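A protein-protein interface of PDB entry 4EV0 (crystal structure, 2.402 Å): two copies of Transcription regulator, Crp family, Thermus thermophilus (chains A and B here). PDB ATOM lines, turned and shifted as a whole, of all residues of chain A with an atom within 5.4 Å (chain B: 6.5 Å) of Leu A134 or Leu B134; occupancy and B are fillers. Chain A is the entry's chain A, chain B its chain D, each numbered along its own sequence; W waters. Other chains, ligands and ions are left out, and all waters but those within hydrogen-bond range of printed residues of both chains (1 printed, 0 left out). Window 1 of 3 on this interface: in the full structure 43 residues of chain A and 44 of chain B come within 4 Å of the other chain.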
ATOM      1  N   HIS A  57     -18.675 -14.056 -28.849  1.00  0.00           N
ATOM      2  CA  HIS A  57     -19.174 -15.197 -28.098  1.00  0.00           C
ATOM      3  C   HIS A  57     -20.326 -15.936 -28.763  1.00  0.00           C
ATOM      4  O   HIS A  57     -21.476 -15.811 -28.346  1.00  0.00           O
ATOM      5  CB  HIS A  57     -19.573 -14.773 -26.685  1.00  0.00           C
ATOM      6  CG  HIS A  57     -18.460 -14.878 -25.693  1.00  0.00           C
ATOM      7  ND1 HIS A  57     -17.738 -13.784 -25.261  1.00  0.00           N
ATOM      8  CD2 HIS A  57     -17.933 -15.950 -25.056  1.00  0.00           C
ATOM      9  CE1 HIS A  57     -16.821 -14.178 -24.396  1.00  0.00           C
ATOM     10  NE2 HIS A  57     -16.917 -15.489 -24.255  1.00  0.00           N
ATOM     11  N   GLU A 129      -8.903 -12.989 -11.287  1.00  0.00           N
ATOM     12  CA  GLU A 129     -10.247 -12.574 -11.683  1.00  0.00           C
ATOM     13  C   GLU A 129     -10.969 -13.706 -12.413  1.00  0.00           C
ATOM     14  O   GLU A 129     -12.170 -13.903 -12.249  1.00  0.00           O
ATOM     15  CB  GLU A 129     -10.196 -11.316 -12.570  1.00  0.00           C
ATOM     16  CG  GLU A 129     -10.193  -9.978 -11.808  1.00  0.00           C
ATOM     17  CD  GLU A 129      -9.655  -8.792 -12.640  1.00  0.00           C
ATOM     18  OE1 GLU A 129      -9.362  -8.965 -13.849  1.00  0.00           O
ATOM     19  OE2 GLU A 129      -9.517  -7.675 -12.080  1.00  0.00           O
ATOM     20  N   ALA A 130     -10.205 -14.452 -13.203  1.00  0.00           N
ATOM     21  CA  ALA A 130     -10.723 -15.511 -14.039  1.00  0.00           C
ATOM     22  C   ALA A 130     -11.149 -16.722 -13.206  1.00  0.00           C
ATOM     23  O   ALA A 130     -12.118 -17.409 -13.543  1.00  0.00           O
ATOM     24  CB  ALA A 130      -9.682 -15.908 -15.076  1.00  0.00           C
ATOM     25  N   ASP A 131     -10.422 -16.981 -12.122  1.00  0.00           N
ATOM     26  CA  ASP A 131     -10.768 -18.057 -11.221  1.00  0.00           C
ATOM     27  C   ASP A 131     -12.047 -17.704 -10.493  1.00  0.00           C
ATOM     28  O   ASP A 131     -12.913 -18.557 -10.284  1.00  0.00           O
ATOM     29  CB  ASP A 131      -9.648 -18.297 -10.212  1.00  0.00           C
ATOM     30  CG  ASP A 131      -8.394 -18.880 -10.853  1.00  0.00           C
ATOM     31  OD1 ASP A 131      -8.478 -19.387 -11.998  1.00  0.00           O
ATOM     32  OD2 ASP A 131      -7.322 -18.829 -10.196  1.00  0.00           O
ATOM     33  N   LEU A 132     -12.165 -16.444 -10.100  1.00  0.00           N
ATOM     34  CA  LEU A 132     -13.390 -15.985  -9.466  1.00  0.00           C
ATOM     35  C   LEU A 132     -14.601 -16.135 -10.404  1.00  0.00           C
ATOM     36  O   LEU A 132     -15.701 -16.455  -9.956  1.00  0.00           O
ATOM     37  CB  LEU A 132     -13.241 -14.541  -8.983  1.00  0.00           C
ATOM     38  CG  LEU A 132     -14.374 -14.083  -8.060  1.00  0.00           C
ATOM     39  CD1 LEU A 132     -14.618 -15.133  -6.967  1.00  0.00           C
ATOM     40  CD2 LEU A 132     -14.068 -12.709  -7.453  1.00  0.00           C
ATOM     41  N   GLU A 133     -14.388 -15.922 -11.700  1.00  0.00           N
ATOM     42  CA  GLU A 133     -15.449 -16.059 -12.694  1.00  0.00           C
ATOM     43  C   GLU A 133     -15.785 -17.520 -12.944  1.00  0.00           C
ATOM     44  O   GLU A 133     -16.947 -17.860 -13.132  1.00  0.00           O
ATOM     45  CB  GLU A 133     -15.069 -15.392 -14.017  1.00  0.00           C
ATOM     46  CG  GLU A 133     -15.109 -13.884 -13.974  1.00  0.00           C
ATOM     47  CD  GLU A 133     -14.894 -13.239 -15.343  1.00  0.00           C
ATOM     48  OE1 GLU A 133     -15.782 -13.424 -16.214  1.00  0.00           O
ATOM     49  OE2 GLU A 133     -13.849 -12.544 -15.538  1.00  0.00           O
ATOM     50  N   LEU A 134     -14.764 -18.375 -12.948  1.00  0.00           N
ATOM     51  CA  LEU A 134     -14.948 -19.813 -13.154  1.00  0.00           C
ATOM     52  C   LEU A 134     -15.624 -20.548 -11.981  1.00  0.00           C
ATOM     53  O   LEU A 134     -16.295 -21.564 -12.191  1.00  0.00           O
ATOM     54  CB  LEU A 134     -13.616 -20.497 -13.503  1.00  0.00           C
ATOM     55  CG  LEU A 134     -13.082 -20.279 -14.923  1.00  0.00           C
ATOM     56  CD1 LEU A 134     -11.800 -21.058 -15.150  1.00  0.00           C
ATOM     57  CD2 LEU A 134     -14.101 -20.684 -15.959  1.00  0.00           C
ATOM     58  N   ASP A 135     -15.421 -20.050 -10.757  1.00  0.00           N
ATOM     59  CA  ASP A 135     -16.185 -20.498  -9.594  1.00  0.00           C
ATOM     60  C   ASP A 135     -17.658 -20.260  -9.907  1.00  0.00           C
ATOM     61  O   ASP A 135     -18.518 -21.111  -9.643  1.00  0.00           O
ATOM     62  CB  ASP A 135     -15.849 -19.662  -8.357  1.00  0.00           C
ATOM     63  CG  ASP A 135     -14.521 -20.031  -7.707  1.00  0.00           C
ATOM     64  OD1 ASP A 135     -13.913 -21.084  -8.036  1.00  0.00           O
ATOM     65  OD2 ASP A 135     -14.110 -19.248  -6.821  1.00  0.00           O
ATOM     66  N   LEU A 136     -17.930 -19.079 -10.461  1.00  0.00           N
ATOM     67  CA  LEU A 136     -19.280 -18.659 -10.808  1.00  0.00           C
ATOM     68  C   LEU A 136     -19.872 -19.472 -11.950  1.00  0.00           C
ATOM     69  O   LEU A 136     -21.072 -19.724 -11.960  1.00  0.00           O
ATOM     70  CB  LEU A 136     -19.319 -17.166 -11.138  1.00  0.00           C
ATOM     71  CG  LEU A 136     -19.250 -16.271  -9.900  1.00  0.00           C
ATOM     72  CD1 LEU A 136     -18.980 -14.818 -10.264  1.00  0.00           C
ATOM     73  CD2 LEU A 136     -20.543 -16.404  -9.107  1.00  0.00           C
ATOM     74  N   LEU A 137     -19.037 -19.910 -12.885  1.00  0.00           N
ATOM     75  CA  LEU A 137     -19.529 -20.723 -13.993  1.00  0.00           C
ATOM     76  C   LEU A 137     -20.087 -22.060 -13.531  1.00  0.00           C
ATOM     77  O   LEU A 137     -21.098 -22.509 -14.058  1.00  0.00           O
ATOM     78  CB  LEU A 137     -18.449 -20.974 -15.042  1.00  0.00           C
ATOM     79  CG  LEU A 137     -19.041 -20.955 -16.456  1.00  0.00           C
ATOM     80  CD1 LEU A 137     -19.052 -19.505 -16.965  1.00  0.00           C
ATOM     81  CD2 LEU A 137     -18.312 -21.892 -17.427  1.00  0.00           C
ATOM     82  N   SER A 138     -19.409 -22.696 -12.575  1.00  0.00           N
ATOM     83  CA  SER A 138     -19.865 -23.957 -12.002  1.00  0.00           C
ATOM     84  C   SER A 138     -21.276 -23.805 -11.512  1.00  0.00           C
ATOM     85  O   SER A 138     -22.163 -24.598 -11.859  1.00  0.00           O
ATOM     86  CB  SER A 138     -19.003 -24.365 -10.811  1.00  0.00           C
ATOM     87  OG  SER A 138     -17.939 -25.200 -11.217  1.00  0.00           O
ATOM     88  N   HIS B  57     -15.484 -23.471  -2.678  1.00  0.00           N
ATOM     89  CA  HIS B  57     -16.643 -22.599  -2.796  1.00  0.00           C
ATOM     90  C   HIS B  57     -17.938 -23.402  -2.554  1.00  0.00           C
ATOM     91  O   HIS B  57     -17.897 -24.621  -2.356  1.00  0.00           O
ATOM     92  CB  HIS B  57     -16.651 -21.910  -4.169  1.00  0.00           C
ATOM     93  CG  HIS B  57     -16.905 -22.840  -5.322  1.00  0.00           C
ATOM     94  ND1 HIS B  57     -17.515 -22.424  -6.488  1.00  0.00           N
ATOM     95  CD2 HIS B  57     -16.633 -24.156  -5.490  1.00  0.00           C
ATOM     96  CE1 HIS B  57     -17.616 -23.448  -7.320  1.00  0.00           C
ATOM     97  NE2 HIS B  57     -17.094 -24.512  -6.740  1.00  0.00           N
ATOM     98  N   ARG B  63     -13.311 -27.558  -6.219  1.00  0.00           N
ATOM     99  CA  ARG B  63     -13.199 -27.644  -7.659  1.00  0.00           C
ATOM    100  C   ARG B  63     -11.727 -27.778  -8.012  1.00  0.00           C
ATOM    101  O   ARG B  63     -10.973 -26.818  -7.898  1.00  0.00           O
ATOM    102  CB  ARG B  63     -13.791 -26.389  -8.300  1.00  0.00           C
ATOM    103  CG  ARG B  63     -13.646 -26.340  -9.810  1.00  0.00           C
ATOM    104  CD  ARG B  63     -14.442 -25.185 -10.413  1.00  0.00           C
ATOM    105  NE  ARG B  63     -13.927 -23.890  -9.982  1.00  0.00           N
ATOM    106  CZ  ARG B  63     -12.946 -23.253 -10.601  1.00  0.00           C
ATOM    107  NH1 ARG B  63     -12.378 -23.799 -11.671  1.00  0.00           N
ATOM    108  NH2 ARG B  63     -12.535 -22.075 -10.155  1.00  0.00           N
ATOM    109  N   GLU B 129      -6.487 -21.364 -21.554  1.00  0.00           N
ATOM    110  CA  GLU B 129      -7.220 -22.538 -21.096  1.00  0.00           C
ATOM    111  C   GLU B 129      -8.489 -22.134 -20.340  1.00  0.00           C
ATOM    112  O   GLU B 129      -9.527 -22.792 -20.436  1.00  0.00           O
ATOM    113  CB  GLU B 129      -6.303 -23.418 -20.241  1.00  0.00           C
ATOM    114  CG  GLU B 129      -5.166 -24.016 -21.056  1.00  0.00           C
ATOM    115  CD  GLU B 129      -4.033 -24.580 -20.211  1.00  0.00           C
ATOM    116  OE1 GLU B 129      -4.075 -24.449 -18.964  1.00  0.00           O
ATOM    117  OE2 GLU B 129      -3.086 -25.147 -20.804  1.00  0.00           O
ATOM    118  N   ALA B 130      -8.397 -21.031 -19.609  1.00  0.00           N
ATOM    119  CA  ALA B 130      -9.554 -20.477 -18.911  1.00  0.00           C
ATOM    120  C   ALA B 130     -10.633 -19.899 -19.839  1.00  0.00           C
ATOM    121  O   ALA B 130     -11.814 -20.050 -19.555  1.00  0.00           O
ATOM    122  CB  ALA B 130      -9.118 -19.443 -17.892  1.00  0.00           C
ATOM    123  N   ASP B 131     -10.242 -19.229 -20.925  1.00  0.00           N
ATOM    124  CA  ASP B 131     -11.222 -18.710 -21.885  1.00  0.00           C
ATOM    125  C   ASP B 131     -11.976 -19.877 -22.523  1.00  0.00           C
ATOM    126  O   ASP B 131     -13.180 -19.788 -22.788  1.00  0.00           O
ATOM    127  CB  ASP B 131     -10.560 -17.856 -22.981  1.00  0.00           C
ATOM    128  CG  ASP B 131     -10.246 -16.420 -22.524  1.00  0.00           C
ATOM    129  OD1 ASP B 131     -11.129 -15.780 -21.906  1.00  0.00           O
ATOM    130  OD2 ASP B 131      -9.117 -15.928 -22.791  1.00  0.00           O
ATOM    131  N   LEU B 132     -11.261 -20.978 -22.750  1.00  0.00           N
ATOM    132  CA  LEU B 132     -11.855 -22.195 -23.316  1.00  0.00           C
ATOM    133  C   LEU B 132     -12.895 -22.838 -22.394  1.00  0.00           C
ATOM    134  O   LEU B 132     -13.955 -23.284 -22.855  1.00  0.00           O
ATOM    135  CB  LEU B 132     -10.776 -23.232 -23.646  1.00  0.00           C
ATOM    136  CG  LEU B 132      -9.773 -22.865 -24.742  1.00  0.00           C
ATOM    137  CD1 LEU B 132      -8.515 -23.726 -24.667  1.00  0.00           C
ATOM    138  CD2 LEU B 132     -10.430 -22.963 -26.120  1.00  0.00           C
ATOM    139  N   GLU B 133     -12.584 -22.890 -21.100  1.00  0.00           N
ATOM    140  CA  GLU B 133     -13.484 -23.483 -20.116  1.00  0.00           C
ATOM    141  C   GLU B 133     -14.787 -22.679 -20.017  1.00  0.00           C
ATOM    142  O   GLU B 133     -15.846 -23.223 -19.702  1.00  0.00           O
ATOM    143  CB  GLU B 133     -12.784 -23.611 -18.750  1.00  0.00           C
ATOM    144  CG  GLU B 133     -13.258 -24.804 -17.904  1.00  0.00           C
ATOM    145  CD  GLU B 133     -12.501 -24.954 -16.571  1.00  0.00           C
ATOM    146  OE1 GLU B 133     -13.066 -25.573 -15.634  1.00  0.00           O
ATOM    147  OE2 GLU B 133     -11.348 -24.462 -16.457  1.00  0.00           O
ATOM    148  N   LEU B 134     -14.704 -21.387 -20.311  1.00  0.00           N
ATOM    149  CA  LEU B 134     -15.884 -20.533 -20.360  1.00  0.00           C
ATOM    150  C   LEU B 134     -16.830 -20.953 -21.486  1.00  0.00           C
ATOM    151  O   LEU B 134     -18.051 -20.972 -21.315  1.00  0.00           O
ATOM    152  CB  LEU B 134     -15.463 -19.071 -20.531  1.00  0.00           C
ATOM    153  CG  LEU B 134     -14.701 -18.520 -19.323  1.00  0.00           C
ATOM    154  CD1 LEU B 134     -14.001 -17.199 -19.638  1.00  0.00           C
ATOM    155  CD2 LEU B 134     -15.650 -18.362 -18.149  1.00  0.00           C
ATOM    156  N   ASP B 135     -16.253 -21.309 -22.629  1.00  0.00           N
ATOM    157  CA  ASP B 135     -17.028 -21.584 -23.833  1.00  0.00           C
ATOM    158  C   ASP B 135     -17.519 -23.041 -23.935  1.00  0.00           C
ATOM    159  O   ASP B 135     -18.290 -23.378 -24.834  1.00  0.00           O
ATOM    160  CB  ASP B 135     -16.206 -21.212 -25.083  1.00  0.00           C
ATOM    161  CG  ASP B 135     -15.839 -19.717 -25.146  1.00  0.00           C
ATOM    162  OD1 ASP B 135     -16.672 -18.867 -24.757  1.00  0.00           O
ATOM    163  OD2 ASP B 135     -14.715 -19.392 -25.599  1.00  0.00           O
ATOM    164  N   LEU B 136     -17.094 -23.895 -23.008  1.00  0.00           N
ATOM    165  CA  LEU B 136     -17.284 -25.345 -23.147  1.00  0.00           C
ATOM    166  C   LEU B 136     -18.659 -25.880 -22.694  1.00  0.00           C
ATOM    167  O   LEU B 136     -19.217 -25.438 -21.685  1.00  0.00           O
ATOM    168  CB  LEU B 136     -16.142 -26.084 -22.438  1.00  0.00           C
ATOM    169  CG  LEU B 136     -16.096 -27.610 -22.415  1.00  0.00           C
ATOM    170  CD1 LEU B 136     -14.660 -28.077 -22.541  1.00  0.00           C
ATOM    171  CD2 LEU B 136     -16.696 -28.133 -21.121  1.00  0.00           C
ATOM    172  N   LEU B 137     -19.186 -26.835 -23.462  1.00  0.00           N
ATOM    173  CA  LEU B 137     -20.479 -27.472 -23.197  1.00  0.00           C
ATOM    174  C   LEU B 137     -20.495 -28.875 -23.808  1.00  0.00           C
ATOM    175  O   LEU B 137     -19.993 -29.069 -24.920  1.00  0.00           O
ATOM    176  CB  LEU B 137     -21.615 -26.637 -23.799  1.00  0.00           C
ATOM    177  CG  LEU B 137     -23.057 -27.175 -23.767  1.00  0.00           C
ATOM    178  CD1 LEU B 137     -23.636 -27.223 -22.346  1.00  0.00           C
ATOM    179  CD2 LEU B 137     -23.960 -26.360 -24.695  1.00  0.00           C
HETATM  180  O   HOH W   1     -10.371 -21.859 -12.409  1.00  0.00           O
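A ring nitrogen (NE2) of His A57 lies close to the side-chain carboxylate (OD1) of Asp B135 (3.4 Å). The side-chain carboxylate (OD1) of Asp A135 lies within salt-bridge range of the guanidinium group (NH2) of Arg B63.
Among the printed residues, pairs that only touch across the chains: Asp A135 with His B57 (3.4 Å), Asp A131 with Arg B63 (3.5 Å), Leu A134 with Leu B134 (3.5 Å), Ser A138 with Arg B63 (3.6 Å), Leu A137 with Glu B133 (3.6 Å), Leu A134 with Glu B133 (3.7 Å), Leu A137 with Leu B134 (3.8 Å), Leu A134 with Arg B63 (3.9 Å) and Ser A138 with His B57 (3.9 Å).
Of chain A, only Leu A134 and Leu A137 come within 4 Å of Leu B134. Of the printed residues of chain A, Glu B133 touches Leu A134 (3.7 Å) and Leu A137 (3.6 Å). Of the printed residues of chain A, Asp B135 touches His A57 (3.2 Å). Printed residues of chain B within 4 Å of Leu A137: Glu B133 and Leu B134. Leu A136 touches none of the printed residues of chain B. The nearest residue of chain B that does not touch Leu A134 is Ala B130 (4.2 Å). The nearest residue of chain A that does not touch Leu B134 is Glu A133 (5.1 Å). The nearest printed residue of chain A that does not touch Asp B135 is Leu A137 (5.6 Å).
Hydrophobic or aromatic side chains of chain B that line the printed part of chain A: His B57 and Leu B134. Hydrophobic or aromatic side chains of chain A within 4 Å of the printed part of chain B: His A57, Leu A134 and Leu A137. Among the printed residues, 11 pairs touch across the chains. Among the printed residues, Asp or Glu carboxylates within 4 Å of a Lys or Arg side-chain nitrogen of the other chain: Asp A135 with Arg B63.
His A57 touches Asp B135, and with the chains exchanged Asp A135 touches His B57. Leu A134 touches its own counterpart, Leu B134. Leu A137 touches Glu B133, but with the chains exchanged Glu A133 does not touch Leu B137 (13.9 Å). Leu A137 touches Leu B134, but with the chains exchanged Leu A134 does not touch Leu B137 (11.0 Å). Positions printed for both chains: 57, 129, 130, 131, 132, 133, 134, 135, 136 and 137. Of the 11 pairs that touch across the chains among the printed residues, 3 have their exchanged pair printed and touching as well.
Water W1 bridges the guanidinium group of Arg B63 (2.9 Å) and the side-chain carboxylate of Asp A131 (3.1 Å).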
